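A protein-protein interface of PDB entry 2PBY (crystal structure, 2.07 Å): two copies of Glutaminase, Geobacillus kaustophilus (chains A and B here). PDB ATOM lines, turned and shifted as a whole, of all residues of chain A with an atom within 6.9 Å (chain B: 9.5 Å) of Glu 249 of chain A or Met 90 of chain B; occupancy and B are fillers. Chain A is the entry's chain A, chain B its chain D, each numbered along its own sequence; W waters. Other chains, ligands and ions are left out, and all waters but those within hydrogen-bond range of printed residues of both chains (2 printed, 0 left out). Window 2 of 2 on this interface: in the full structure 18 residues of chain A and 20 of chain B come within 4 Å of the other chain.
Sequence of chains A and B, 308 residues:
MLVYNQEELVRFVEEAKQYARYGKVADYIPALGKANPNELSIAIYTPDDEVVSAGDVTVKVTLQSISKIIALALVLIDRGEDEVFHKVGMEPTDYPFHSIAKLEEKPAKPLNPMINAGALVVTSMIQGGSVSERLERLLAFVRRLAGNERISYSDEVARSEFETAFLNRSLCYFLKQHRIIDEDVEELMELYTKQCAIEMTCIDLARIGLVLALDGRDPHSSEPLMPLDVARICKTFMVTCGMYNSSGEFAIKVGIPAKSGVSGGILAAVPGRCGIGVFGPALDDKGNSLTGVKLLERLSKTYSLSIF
Printed residues of chain B within 4 Å of Ser 246 of chain A: Glu 91 (3.2 Å).
Glu 249 of chain A touches just these residues of chain B: Met 90 and Glu 91.
Ile 252 of chain A touches just these residues of chain B: Glu 81 (3.8 Å), Met 90 (3.8 Å), Ile 233 (3.9 Å) and Thr 236 (3.6 Å).
Of the printed residues of chain A, Glu 81 of chain B touches Ile 252 (3.8 Å).
Printed residues of chain A within 4 Å of Thr 236 of chain B: Ala 251 (3.6 Å) and Ile 252 (3.6 Å).
Cys 241 of chain B touches none of the printed residues of chain A.
The nearest residue of chain B that does not touch Glu 249 of chain A is Pro 92 of chain B (6.3 Å).
The nearest printed residue of chain B that does not touch Ser 246 of chain A is Pro 92 of chain B (6.7 Å).
The backbone carbonyl oxygen of Thr 236 of chain B is in hydrogen-bond range of the side-chain hydroxyl of Thr 240 of chain B (3.2 Å).
O of Asn 245 of chain A is in hydrogen-bond range of NZ of Lys 286 of chain A, 3.0 Å away.
The backbone carbonyl oxygen (O) of Ile 233 of chain B lies within hydrogen-bond range of the side-chain hydroxyl (OG1) of Thr 236 of chain B, 2.7 Å away.
Printed residues of chain B that touch a printed residue of chain A: Glu 81, Met 90, Glu 91, Ile 233 and Thr 236.
Printed residues of chain A that touch a printed residue of chain B: Asn 245, Ser 246, Ser 247, Gly 248, Glu 249, Ala 251 and Ile 252.
Hydrophobic or aromatic side chains of chain A within 4 Å of the printed part of chain B: Ile 252.
Among the printed residues, 12 pairs touch across the chains.
Water W2 lies within hydrogen-bond range of OE2 of Glu 91 of chain B (2.4 Å), NZ of Lys 286 of chain A (3.2 Å) and OE1 of Glu 249 of chain A (3.4 Å).
Water W1 bridges the side-chain hydroxyl (OG1) of Thr 236 of chain B (2.8 Å) and the backbone carbonyl oxygen (O) of Gly 248 of chain A (2.9 Å).
No position is printed for both chains.
The side-chain carboxylate (OE2) of Glu 91 of chain B sits at hydrogen-bond distance from the backbone NH (N) of Glu 249 of chain A (3.1 Å).
The backbone NH of Ser 247 of chain A sits at hydrogen-bond distance from the side-chain carboxylate of Glu 91 of chain B, at 3.2 Å.
N of Gly 248 of chain A sits at hydrogen-bond distance from OE1 of Glu 91 of chain B (2.7 Å).
Asn 245 of chain A touches Glu 91 of chain B (O to CD, 3.4 Å).
Ser 246 of chain A touches Glu 91 of chain B (CA to OE2, 3.2 Å).
Gly 248 of chain A touches Met 90 of chain B (CA to O, 3.3 Å).
Glu 249 of chain A touches Met 90 of chain B (CG to CE, 3.8 Å).
CG2 of Thr 236 of chain B touches O of Ala 251 of chain A, at 3.6 Å.
Ile 252 of chain A touches Glu 81 of chain B.
SD of Met 90 of chain B touches CD1 of Ile 252 of chain A, at 3.8 Å.
CG2 of Ile 252 of chain A touches CG1 of Ile 233 of chain B, at 3.9 Å.
Ile 252 of chain A touches Thr 236 of chain B.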
ATOM      1  N   ASN A 245      19.604  20.369 -28.558  1.00  0.00           N
ATOM      2  CA  ASN A 245      18.251  20.157 -29.050  1.00  0.00           C
ATOM      3  C   ASN A 245      17.617  18.925 -28.435  1.00  0.00           C
ATOM      4  O   ASN A 245      16.648  18.376 -28.966  1.00  0.00           O
ATOM      5  CB  ASN A 245      18.213  20.095 -30.602  1.00  0.00           C
ATOM      6  CG  ASN A 245      18.680  21.420 -31.246  1.00  0.00           C
ATOM      7  OD1 ASN A 245      19.507  21.433 -32.196  1.00  0.00           O
ATOM      8  ND2 ASN A 245      18.204  22.542 -30.684  1.00  0.00           N
ATOM      9  N   SER A 246      18.128  18.487 -27.295  1.00  0.00           N
ATOM     10  CA  SER A 246      17.480  17.360 -26.688  1.00  0.00           C
ATOM     11  C   SER A 246      17.358  17.457 -25.164  1.00  0.00           C
ATOM     12  O   SER A 246      17.452  16.460 -24.478  1.00  0.00           O
ATOM     13  CB  SER A 246      18.158  16.071 -27.132  1.00  0.00           C
ATOM     14  OG  SER A 246      19.534  16.163 -26.967  1.00  0.00           O
ATOM     15  N   SER A 247      17.103  18.645 -24.649  1.00  0.00           N
ATOM     16  CA  SER A 247      16.910  18.778 -23.218  1.00  0.00           C
ATOM     17  C   SER A 247      15.727  17.984 -22.687  1.00  0.00           C
ATOM     18  O   SER A 247      15.788  17.490 -21.577  1.00  0.00           O
ATOM     19  CB  SER A 247      16.694  20.257 -22.818  1.00  0.00           C
ATOM     20  OG  SER A 247      17.792  21.008 -23.293  1.00  0.00           O
ATOM     21  N   GLY A 248      14.641  17.930 -23.459  1.00  0.00           N
ATOM     22  CA  GLY A 248      13.406  17.247 -23.041  1.00  0.00           C
ATOM     23  C   GLY A 248      13.653  15.736 -22.903  1.00  0.00           C
ATOM     24  O   GLY A 248      13.242  15.134 -21.933  1.00  0.00           O
ATOM     25  N   GLU A 249      14.344  15.159 -23.882  1.00  0.00           N
ATOM     26  CA  GLU A 249      14.759  13.759 -23.835  1.00  0.00           C
ATOM     27  C   GLU A 249      15.706  13.484 -22.681  1.00  0.00           C
ATOM     28  O   GLU A 249      15.560  12.455 -22.026  1.00  0.00           O
ATOM     29  CB  GLU A 249      15.476  13.357 -25.151  1.00  0.00           C
ATOM     30  CG  GLU A 249      15.643  11.859 -25.300  1.00  0.00           C
ATOM     31  CD  GLU A 249      16.392  11.474 -26.590  1.00  0.00           C
ATOM     32  OE1 GLU A 249      16.644  12.382 -27.406  1.00  0.00           O
ATOM     33  OE2 GLU A 249      16.743  10.273 -26.779  1.00  0.00           O
ATOM     34  N   PHE A 250      16.699  14.372 -22.460  1.00  0.00           N
ATOM     35  CA  PHE A 250      17.628  14.251 -21.307  1.00  0.00           C
ATOM     36  C   PHE A 250      16.913  14.361 -19.936  1.00  0.00           C
ATOM     37  O   PHE A 250      17.230  13.632 -18.970  1.00  0.00           O
ATOM     38  CB  PHE A 250      18.732  15.317 -21.430  1.00  0.00           C
ATOM     39  CG  PHE A 250      19.807  15.230 -20.367  1.00  0.00           C
ATOM     40  CD1 PHE A 250      20.954  14.459 -20.585  1.00  0.00           C
ATOM     41  CD2 PHE A 250      19.675  15.911 -19.173  1.00  0.00           C
ATOM     42  CE1 PHE A 250      21.958  14.365 -19.629  1.00  0.00           C
ATOM     43  CE2 PHE A 250      20.660  15.801 -18.183  1.00  0.00           C
ATOM     44  CZ  PHE A 250      21.814  15.057 -18.403  1.00  0.00           C
ATOM     45  N   ALA A 251      15.925  15.258 -19.821  1.00  0.00           N
ATOM     46  CA  ALA A 251      15.092  15.308 -18.601  1.00  0.00           C
ATOM     47  C   ALA A 251      14.383  13.947 -18.308  1.00  0.00           C
ATOM     48  O   ALA A 251      14.294  13.529 -17.156  1.00  0.00           O
ATOM     49  CB  ALA A 251      14.021  16.486 -18.687  1.00  0.00           C
ATOM     50  N   ILE A 252      13.898  13.283 -19.350  1.00  0.00           N
ATOM     51  CA  ILE A 252      13.166  12.009 -19.236  1.00  0.00           C
ATOM     52  C   ILE A 252      14.142  10.863 -18.876  1.00  0.00           C
ATOM     53  O   ILE A 252      13.896  10.117 -17.936  1.00  0.00           O
ATOM     54  CB  ILE A 252      12.421  11.704 -20.568  1.00  0.00           C
ATOM     55  CG1 ILE A 252      11.133  12.535 -20.642  1.00  0.00           C
ATOM     56  CG2 ILE A 252      11.967  10.237 -20.686  1.00  0.00           C
ATOM     57  CD1 ILE A 252      10.517  12.470 -22.039  1.00  0.00           C
ATOM     58  N   LYS A 253      15.268  10.800 -19.574  1.00  0.00           N
ATOM     59  CA  LYS A 253      16.227   9.711 -19.460  1.00  0.00           C
ATOM     60  C   LYS A 253      17.291   9.913 -18.405  1.00  0.00           C
ATOM     61  O   LYS A 253      17.903   8.931 -17.942  1.00  0.00           O
ATOM     62  CB  LYS A 253      16.923   9.514 -20.794  1.00  0.00           C
ATOM     63  CG  LYS A 253      15.942   9.251 -21.925  1.00  0.00           C
ATOM     64  CD  LYS A 253      16.668   8.884 -23.201  1.00  0.00           C
ATOM     65  CE  LYS A 253      15.702   8.415 -24.290  1.00  0.00           C
ATOM     66  NZ  LYS A 253      14.690   7.542 -23.727  1.00  0.00           N
ATOM     67  N   VAL A 254      17.523  11.152 -17.990  1.00  0.00           N
ATOM     68  CA  VAL A 254      18.497  11.377 -16.921  1.00  0.00           C
ATOM     69  C   VAL A 254      17.931  12.195 -15.753  1.00  0.00           C
ATOM     70  O   VAL A 254      18.147  11.843 -14.578  1.00  0.00           O
ATOM     71  CB  VAL A 254      19.841  12.023 -17.510  1.00  0.00           C
ATOM     72  CG1 VAL A 254      20.911  12.158 -16.402  1.00  0.00           C
ATOM     73  CG2 VAL A 254      20.327  11.179 -18.623  1.00  0.00           C
ATOM     74  N   GLY A 255      17.253  13.297 -16.082  1.00  0.00           N
ATOM     75  CA  GLY A 255      16.564  14.104 -15.089  1.00  0.00           C
ATOM     76  C   GLY A 255      17.352  14.984 -14.138  1.00  0.00           C
ATOM     77  O   GLY A 255      16.884  15.272 -13.044  1.00  0.00           O
ATOM     78  N   ASP A 284      26.789  11.987 -30.180  1.00  0.00           N
ATOM     79  CA  ASP A 284      25.677  11.435 -30.916  1.00  0.00           C
ATOM     80  C   ASP A 284      25.288  12.300 -32.147  1.00  0.00           C
ATOM     81  O   ASP A 284      25.888  13.377 -32.375  1.00  0.00           O
ATOM     82  CB  ASP A 284      24.482  11.221 -29.973  1.00  0.00           C
ATOM     83  CG  ASP A 284      23.975  12.509 -29.319  1.00  0.00           C
ATOM     84  OD1 ASP A 284      24.069  13.615 -29.935  1.00  0.00           O
ATOM     85  OD2 ASP A 284      23.474  12.392 -28.155  1.00  0.00           O
ATOM     86  N   LYS A 286      23.055  14.242 -32.525  1.00  0.00           N
ATOM     87  CA  LYS A 286      22.473  15.507 -32.152  1.00  0.00           C
ATOM     88  C   LYS A 286      23.445  16.404 -31.387  1.00  0.00           C
ATOM     89  O   LYS A 286      23.019  17.343 -30.738  1.00  0.00           O
ATOM     90  CB  LYS A 286      21.232  15.295 -31.296  1.00  0.00           C
ATOM     91  CG  LYS A 286      20.125  14.457 -31.954  1.00  0.00           C
ATOM     92  CD  LYS A 286      18.895  14.359 -30.992  1.00  0.00           C
ATOM     93  CE  LYS A 286      18.012  15.668 -31.039  1.00  0.00           C
ATOM     94  NZ  LYS A 286      16.777  15.629 -30.191  1.00  0.00           N
ATOM     95  N   GLU A 297      23.132   8.419 -17.870  1.00  0.00           N
ATOM     96  CA  GLU A 297      21.895   7.613 -17.744  1.00  0.00           C
ATOM     97  C   GLU A 297      22.060   6.471 -16.751  1.00  0.00           C
ATOM     98  O   GLU A 297      21.216   6.256 -15.875  1.00  0.00           O
ATOM     99  CB  GLU A 297      21.437   7.065 -19.095  1.00  0.00           C
ATOM    100  CG  GLU A 297      21.023   8.112 -20.121  1.00  0.00           C
ATOM    101  CD  GLU A 297      20.676   7.514 -21.498  1.00  0.00           C
ATOM    102  OE1 GLU A 297      20.933   6.307 -21.718  1.00  0.00           O
ATOM    103  OE2 GLU A 297      20.139   8.252 -22.358  1.00  0.00           O
ATOM    104  N   LEU B  72      -1.996  12.426 -21.807  1.00  0.00           N
ATOM    105  CA  LEU B  72      -0.654  11.854 -22.111  1.00  0.00           C
ATOM    106  C   LEU B  72      -0.314  10.655 -21.230  1.00  0.00           C
ATOM    107  O   LEU B  72       0.104   9.634 -21.756  1.00  0.00           O
ATOM    108  CB  LEU B  72       0.430  12.897 -21.933  1.00  0.00           C
ATOM    109  CG  LEU B  72       1.839  12.378 -22.207  1.00  0.00           C
ATOM    110  CD1 LEU B  72       2.058  11.942 -23.645  1.00  0.00           C
ATOM    111  CD2 LEU B  72       2.762  13.533 -21.821  1.00  0.00           C
ATOM    112  N   LEU B  76       0.385   6.946 -22.654  1.00  0.00           N
ATOM    113  CA  LEU B  76       1.639   6.293 -22.275  1.00  0.00           C
ATOM    114  C   LEU B  76       1.404   4.943 -21.596  1.00  0.00           C
ATOM    115  O   LEU B  76       2.091   3.971 -21.947  1.00  0.00           O
ATOM    116  CB  LEU B  76       2.495   7.187 -21.376  1.00  0.00           C
ATOM    117  CG  LEU B  76       3.198   8.355 -22.073  1.00  0.00           C
ATOM    118  CD1 LEU B  76       3.745   9.281 -21.013  1.00  0.00           C
ATOM    119  CD2 LEU B  76       4.328   7.865 -23.020  1.00  0.00           C
ATOM    120  N   GLU B  81       5.787   4.125 -23.999  1.00  0.00           N
ATOM    121  CA  GLU B  81       6.723   5.205 -24.273  1.00  0.00           C
ATOM    122  C   GLU B  81       7.178   5.206 -25.725  1.00  0.00           C
ATOM    123  O   GLU B  81       7.292   6.251 -26.382  1.00  0.00           O
ATOM    124  CB  GLU B  81       7.922   4.978 -23.341  1.00  0.00           C
ATOM    125  CG  GLU B  81       9.125   5.897 -23.481  1.00  0.00           C
ATOM    126  CD  GLU B  81       9.888   6.059 -22.155  1.00  0.00           C
ATOM    127  OE1 GLU B  81       9.556   5.339 -21.177  1.00  0.00           O
ATOM    128  OE2 GLU B  81      10.815   6.917 -22.089  1.00  0.00           O
ATOM    129  N   ASP B  82       7.401   4.004 -26.231  1.00  0.00           N
ATOM    130  CA  ASP B  82       7.977   3.819 -27.548  1.00  0.00           C
ATOM    131  C   ASP B  82       7.093   4.322 -28.641  1.00  0.00           C
ATOM    132  O   ASP B  82       7.545   5.096 -29.462  1.00  0.00           O
ATOM    133  CB  ASP B  82       8.314   2.351 -27.813  1.00  0.00           C
ATOM    134  CG  ASP B  82       9.345   2.206 -28.930  1.00  0.00           C
ATOM    135  OD1 ASP B  82       8.917   2.086 -30.107  1.00  0.00           O
ATOM    136  OD2 ASP B  82      10.562   2.266 -28.617  1.00  0.00           O
ATOM    137  N   VAL B  84       4.431   6.225 -28.257  1.00  0.00           N
ATOM    138  CA  VAL B  84       3.974   7.611 -28.030  1.00  0.00           C
ATOM    139  C   VAL B  84       4.962   8.619 -28.625  1.00  0.00           C
ATOM    140  O   VAL B  84       4.600   9.495 -29.376  1.00  0.00           O
ATOM    141  CB  VAL B  84       3.608   7.858 -26.515  1.00  0.00           C
ATOM    142  CG1 VAL B  84       3.478   9.316 -26.212  1.00  0.00           C
ATOM    143  CG2 VAL B  84       2.276   7.253 -26.243  1.00  0.00           C
ATOM    144  N   PHE B  85       6.234   8.442 -28.302  1.00  0.00           N
ATOM    145  CA  PHE B  85       7.226   9.361 -28.788  1.00  0.00           C
ATOM    146  C   PHE B  85       7.733   9.115 -30.208  1.00  0.00           C
ATOM    147  O   PHE B  85       8.740   9.675 -30.619  1.00  0.00           O
ATOM    148  CB  PHE B  85       8.324   9.504 -27.750  1.00  0.00           C
ATOM    149  CG  PHE B  85       7.813  10.095 -26.473  1.00  0.00           C
ATOM    150  CD1 PHE B  85       7.140  11.309 -26.483  1.00  0.00           C
ATOM    151  CD2 PHE B  85       7.979   9.440 -25.274  1.00  0.00           C
ATOM    152  CE1 PHE B  85       6.643  11.871 -25.286  1.00  0.00           C
ATOM    153  CE2 PHE B  85       7.519   9.996 -24.071  1.00  0.00           C
ATOM    154  CZ  PHE B  85       6.841  11.193 -24.077  1.00  0.00           C
ATOM    155  N   HIS B  86       7.039   8.247 -30.927  1.00  0.00           N
ATOM    156  CA  HIS B  86       7.123   8.163 -32.391  1.00  0.00           C
ATOM    157  C   HIS B  86       5.984   9.030 -32.959  1.00  0.00           C
ATOM    158  O   HIS B  86       6.108   9.513 -34.071  1.00  0.00           O
ATOM    159  CB  HIS B  86       6.986   6.701 -32.859  1.00  0.00           C
ATOM    160  CG  HIS B  86       6.654   6.539 -34.331  1.00  0.00           C
ATOM    161  ND1 HIS B  86       7.524   6.910 -35.343  1.00  0.00           N
ATOM    162  CD2 HIS B  86       5.557   6.023 -34.949  1.00  0.00           C
ATOM    163  CE1 HIS B  86       6.970   6.634 -36.516  1.00  0.00           C
ATOM    164  NE2 HIS B  86       5.772   6.110 -36.304  1.00  0.00           N
ATOM    165  N   LYS B  87       4.900   9.260 -32.195  1.00  0.00           N
ATOM    166  CA  LYS B  87       3.842  10.163 -32.670  1.00  0.00           C
ATOM    167  C   LYS B  87       4.029  11.659 -32.283  1.00  0.00           C
ATOM    168  O   LYS B  87       3.692  12.551 -33.049  1.00  0.00           O
ATOM    169  CB  LYS B  87       2.461   9.701 -32.187  1.00  0.00           C
ATOM    170  CG  LYS B  87       2.014   8.272 -32.579  1.00  0.00           C
ATOM    171  CD  LYS B  87       1.690   8.155 -34.061  1.00  0.00           C
ATOM    172  CE  LYS B  87       0.554   9.054 -34.502  1.00  0.00           C
ATOM    173  NZ  LYS B  87       0.674   9.278 -35.988  1.00  0.00           N
ATOM    174  N   VAL B  88       4.519  11.917 -31.070  1.00  0.00           N
ATOM    175  CA  VAL B  88       4.657  13.294 -30.544  1.00  0.00           C
ATOM    176  C   VAL B  88       6.101  13.466 -30.061  1.00  0.00           C
ATOM    177  O   VAL B  88       6.824  12.486 -29.898  1.00  0.00           O
ATOM    178  CB  VAL B  88       3.607  13.623 -29.414  1.00  0.00           C
ATOM    179  CG1 VAL B  88       2.143  13.684 -29.978  1.00  0.00           C
ATOM    180  CG2 VAL B  88       3.686  12.707 -28.242  1.00  0.00           C
ATOM    181  N   GLY B  89       6.514  14.698 -29.816  1.00  0.00           N
ATOM    182  CA  GLY B  89       7.889  14.946 -29.484  1.00  0.00           C
ATOM    183  C   GLY B  89       8.103  14.985 -28.001  1.00  0.00           C
ATOM    184  O   GLY B  89       7.150  15.004 -27.224  1.00  0.00           O
ATOM    185  N   MET B  90       9.371  15.015 -27.615  1.00  0.00           N
ATOM    186  CA  MET B  90       9.800  15.209 -26.249  1.00  0.00           C
ATOM    187  C   MET B  90      10.273  16.624 -25.968  1.00  0.00           C
ATOM    188  O   MET B  90      10.611  16.930 -24.833  1.00  0.00           O
ATOM    189  CB  MET B  90      10.949  14.223 -25.901  1.00  0.00           C
ATOM    190  CG  MET B  90      10.473  12.780 -25.825  1.00  0.00           C
ATOM    191  SD  MET B  90      11.736  11.563 -25.493  1.00  0.00           S
ATOM    192  CE  MET B  90      12.414  11.281 -27.146  1.00  0.00           C
ATOM    193  N   GLU B  91      10.334  17.486 -26.968  1.00  0.00           N
ATOM    194  CA  GLU B  91      11.045  18.752 -26.804  1.00  0.00           C
ATOM    195  C   GLU B  91      10.132  19.968 -26.650  1.00  0.00           C
ATOM    196  O   GLU B  91       9.177  20.115 -27.409  1.00  0.00           O
ATOM    197  CB  GLU B  91      12.029  19.026 -27.970  1.00  0.00           C
ATOM    198  CG  GLU B  91      13.192  18.006 -28.163  1.00  0.00           C
ATOM    199  CD  GLU B  91      14.010  17.706 -26.887  1.00  0.00           C
ATOM    200  OE1 GLU B  91      14.248  18.625 -26.089  1.00  0.00           O
ATOM    201  OE2 GLU B  91      14.420  16.532 -26.685  1.00  0.00           O
ATOM    202  N   PRO B  92      10.479  20.871 -25.697  1.00  0.00           N
ATOM    203  CA  PRO B  92       9.765  22.128 -25.573  1.00  0.00           C
ATOM    204  C   PRO B  92       9.871  22.904 -26.853  1.00  0.00           C
ATOM    205  O   PRO B  92       9.151  23.873 -26.977  1.00  0.00           O
ATOM    206  CB  PRO B  92      10.512  22.873 -24.455  1.00  0.00           C
ATOM    207  CG  PRO B  92      11.722  22.080 -24.155  1.00  0.00           C
ATOM    208  CD  PRO B  92      11.548  20.724 -24.689  1.00  0.00           C
ATOM    209  N   LEU B 111       5.751  16.973 -32.798  1.00  0.00           N
ATOM    210  CA  LEU B 111       4.928  17.991 -32.146  1.00  0.00           C
ATOM    211  C   LEU B 111       4.833  17.641 -30.666  1.00  0.00           C
ATOM    212  O   LEU B 111       4.458  16.522 -30.289  1.00  0.00           O
ATOM    213  CB  LEU B 111       3.487  17.965 -32.671  1.00  0.00           C
ATOM    214  CG  LEU B 111       3.239  18.302 -34.148  1.00  0.00           C
ATOM    215  CD1 LEU B 111       1.924  17.684 -34.607  1.00  0.00           C
ATOM    216  CD2 LEU B 111       3.290  19.846 -34.363  1.00  0.00           C
ATOM    217  N   ASN B 112       5.061  18.645 -29.839  1.00  0.00           N
ATOM    218  CA  ASN B 112       5.039  18.472 -28.410  1.00  0.00           C
ATOM    219  C   ASN B 112       3.594  18.213 -27.890  1.00  0.00           C
ATOM    220  O   ASN B 112       2.675  18.874 -28.297  1.00  0.00           O
ATOM    221  CB  ASN B 112       5.654  19.732 -27.810  1.00  0.00           C
ATOM    222  CG  ASN B 112       5.267  19.930 -26.379  1.00  0.00           C
ATOM    223  OD1 ASN B 112       4.481  20.765 -26.055  1.00  0.00           O
ATOM    224  ND2 ASN B 112       5.792  19.114 -25.526  1.00  0.00           N
ATOM    225  N   PRO B 113       3.414  17.292 -26.968  1.00  0.00           N
ATOM    226  CA  PRO B 113       2.050  16.964 -26.489  1.00  0.00           C
ATOM    227  C   PRO B 113       1.363  18.041 -25.591  1.00  0.00           C
ATOM    228  O   PRO B 113       0.208  17.879 -25.235  1.00  0.00           O
ATOM    229  CB  PRO B 113       2.265  15.641 -25.735  1.00  0.00           C
ATOM    230  CG  PRO B 113       3.651  15.752 -25.193  1.00  0.00           C
ATOM    231  CD  PRO B 113       4.450  16.478 -26.271  1.00  0.00           C
ATOM    232  N   MET B 114       2.064  19.131 -25.256  1.00  0.00           N
ATOM    233  CA  MET B 114       1.513  20.193 -24.441  1.00  0.00           C
ATOM    234  C   MET B 114       0.962  21.310 -25.317  1.00  0.00           C
ATOM    235  O   MET B 114       0.241  22.158 -24.834  1.00  0.00           O
ATOM    236  CB  MET B 114       2.574  20.788 -23.469  1.00  0.00           C
ATOM    237  CG  MET B 114       3.083  19.869 -22.354  1.00  0.00           C
ATOM    238  SD  MET B 114       1.776  19.141 -21.287  1.00  0.00           S
ATOM    239  CE  MET B 114       1.438  17.513 -22.010  1.00  0.00           C
ATOM    240  N   ILE B 233       7.744  11.225 -16.553  1.00  0.00           N
ATOM    241  CA  ILE B 233       7.594  11.855 -17.860  1.00  0.00           C
ATOM    242  C   ILE B 233       6.636  13.101 -17.852  1.00  0.00           C
ATOM    243  O   ILE B 233       6.976  14.200 -18.376  1.00  0.00           O
ATOM    244  CB  ILE B 233       7.138  10.834 -18.895  1.00  0.00           C
ATOM    245  CG1 ILE B 233       8.318   9.960 -19.302  1.00  0.00           C
ATOM    246  CG2 ILE B 233       6.560  11.555 -20.130  1.00  0.00           C
ATOM    247  CD1 ILE B 233       7.890   8.697 -19.992  1.00  0.00           C
ATOM    248  N   THR B 236       8.217  16.018 -16.136  1.00  0.00           N
ATOM    249  CA  THR B 236       9.221  16.687 -16.953  1.00  0.00           C
ATOM    250  C   THR B 236       8.592  17.712 -17.905  1.00  0.00           C
ATOM    251  O   THR B 236       9.120  18.858 -18.005  1.00  0.00           O
ATOM    252  CB  THR B 236      10.208  15.724 -17.743  1.00  0.00           C
ATOM    253  OG1 THR B 236       9.511  15.146 -18.838  1.00  0.00           O
ATOM    254  CG2 THR B 236      10.854  14.614 -16.835  1.00  0.00           C
ATOM    255  N   PHE B 237       7.491  17.334 -18.585  1.00  0.00           N
ATOM    256  CA  PHE B 237       6.764  18.282 -19.433  1.00  0.00           C
ATOM    257  C   PHE B 237       6.214  19.425 -18.619  1.00  0.00           C
ATOM    258  O   PHE B 237       6.098  20.515 -19.136  1.00  0.00           O
ATOM    259  CB  PHE B 237       5.605  17.618 -20.215  1.00  0.00           C
ATOM    260  CG  PHE B 237       6.076  16.853 -21.429  1.00  0.00           C
ATOM    261  CD1 PHE B 237       6.562  17.545 -22.574  1.00  0.00           C
ATOM    262  CD2 PHE B 237       6.122  15.467 -21.410  1.00  0.00           C
ATOM    263  CE1 PHE B 237       7.038  16.843 -23.678  1.00  0.00           C
ATOM    264  CE2 PHE B 237       6.624  14.746 -22.540  1.00  0.00           C
ATOM    265  CZ  PHE B 237       7.069  15.424 -23.635  1.00  0.00           C
ATOM    266  N   MET B 238       5.846  19.163 -17.361  1.00  0.00           N
ATOM    267  CA  MET B 238       5.354  20.197 -16.465  1.00  0.00           C
ATOM    268  C   MET B 238       6.444  21.243 -16.084  1.00  0.00           C
ATOM    269  O   MET B 238       6.138  22.350 -15.672  1.00  0.00           O
ATOM    270  CB  MET B 238       4.710  19.578 -15.212  1.00  0.00           C
ATOM    271  CG  MET B 238       3.392  18.855 -15.531  1.00  0.00           C
ATOM    272  SD  MET B 238       2.887  17.818 -14.168  1.00  0.00           S
ATOM    273  CE  MET B 238       2.169  19.057 -13.058  1.00  0.00           C
ATOM    274  N   THR B 240       9.282  21.774 -18.338  1.00  0.00           N
ATOM    275  CA  THR B 240       9.799  22.350 -19.565  1.00  0.00           C
ATOM    276  C   THR B 240       8.806  23.194 -20.344  1.00  0.00           C
ATOM    277  O   THR B 240       9.210  24.110 -21.053  1.00  0.00           O
ATOM    278  CB  THR B 240      10.412  21.305 -20.469  1.00  0.00           C
ATOM    279  OG1 THR B 240       9.396  20.348 -20.839  1.00  0.00           O
ATOM    280  CG2 THR B 240      11.642  20.610 -19.702  1.00  0.00           C
ATOM    281  N   CYS B 241       7.520  22.872 -20.250  1.00  0.00           N
ATOM    282  CA  CYS B 241       6.521  23.576 -21.059  1.00  0.00           C
ATOM    283  C   CYS B 241       5.125  23.444 -20.511  1.00  0.00           C
ATOM    284  O   CYS B 241       4.196  23.302 -21.288  1.00  0.00           O
ATOM    285  CB  CYS B 241       6.527  23.082 -22.507  1.00  0.00           C
ATOM    286  SG  CYS B 241       6.595  21.275 -22.707  1.00  0.00           S
HETATM  287  O   HOH W   1      10.736  16.265 -21.084  1.00  0.00           O
HETATM  288  O   HOH W   2      14.294  14.725 -28.326  1.00  0.00           O
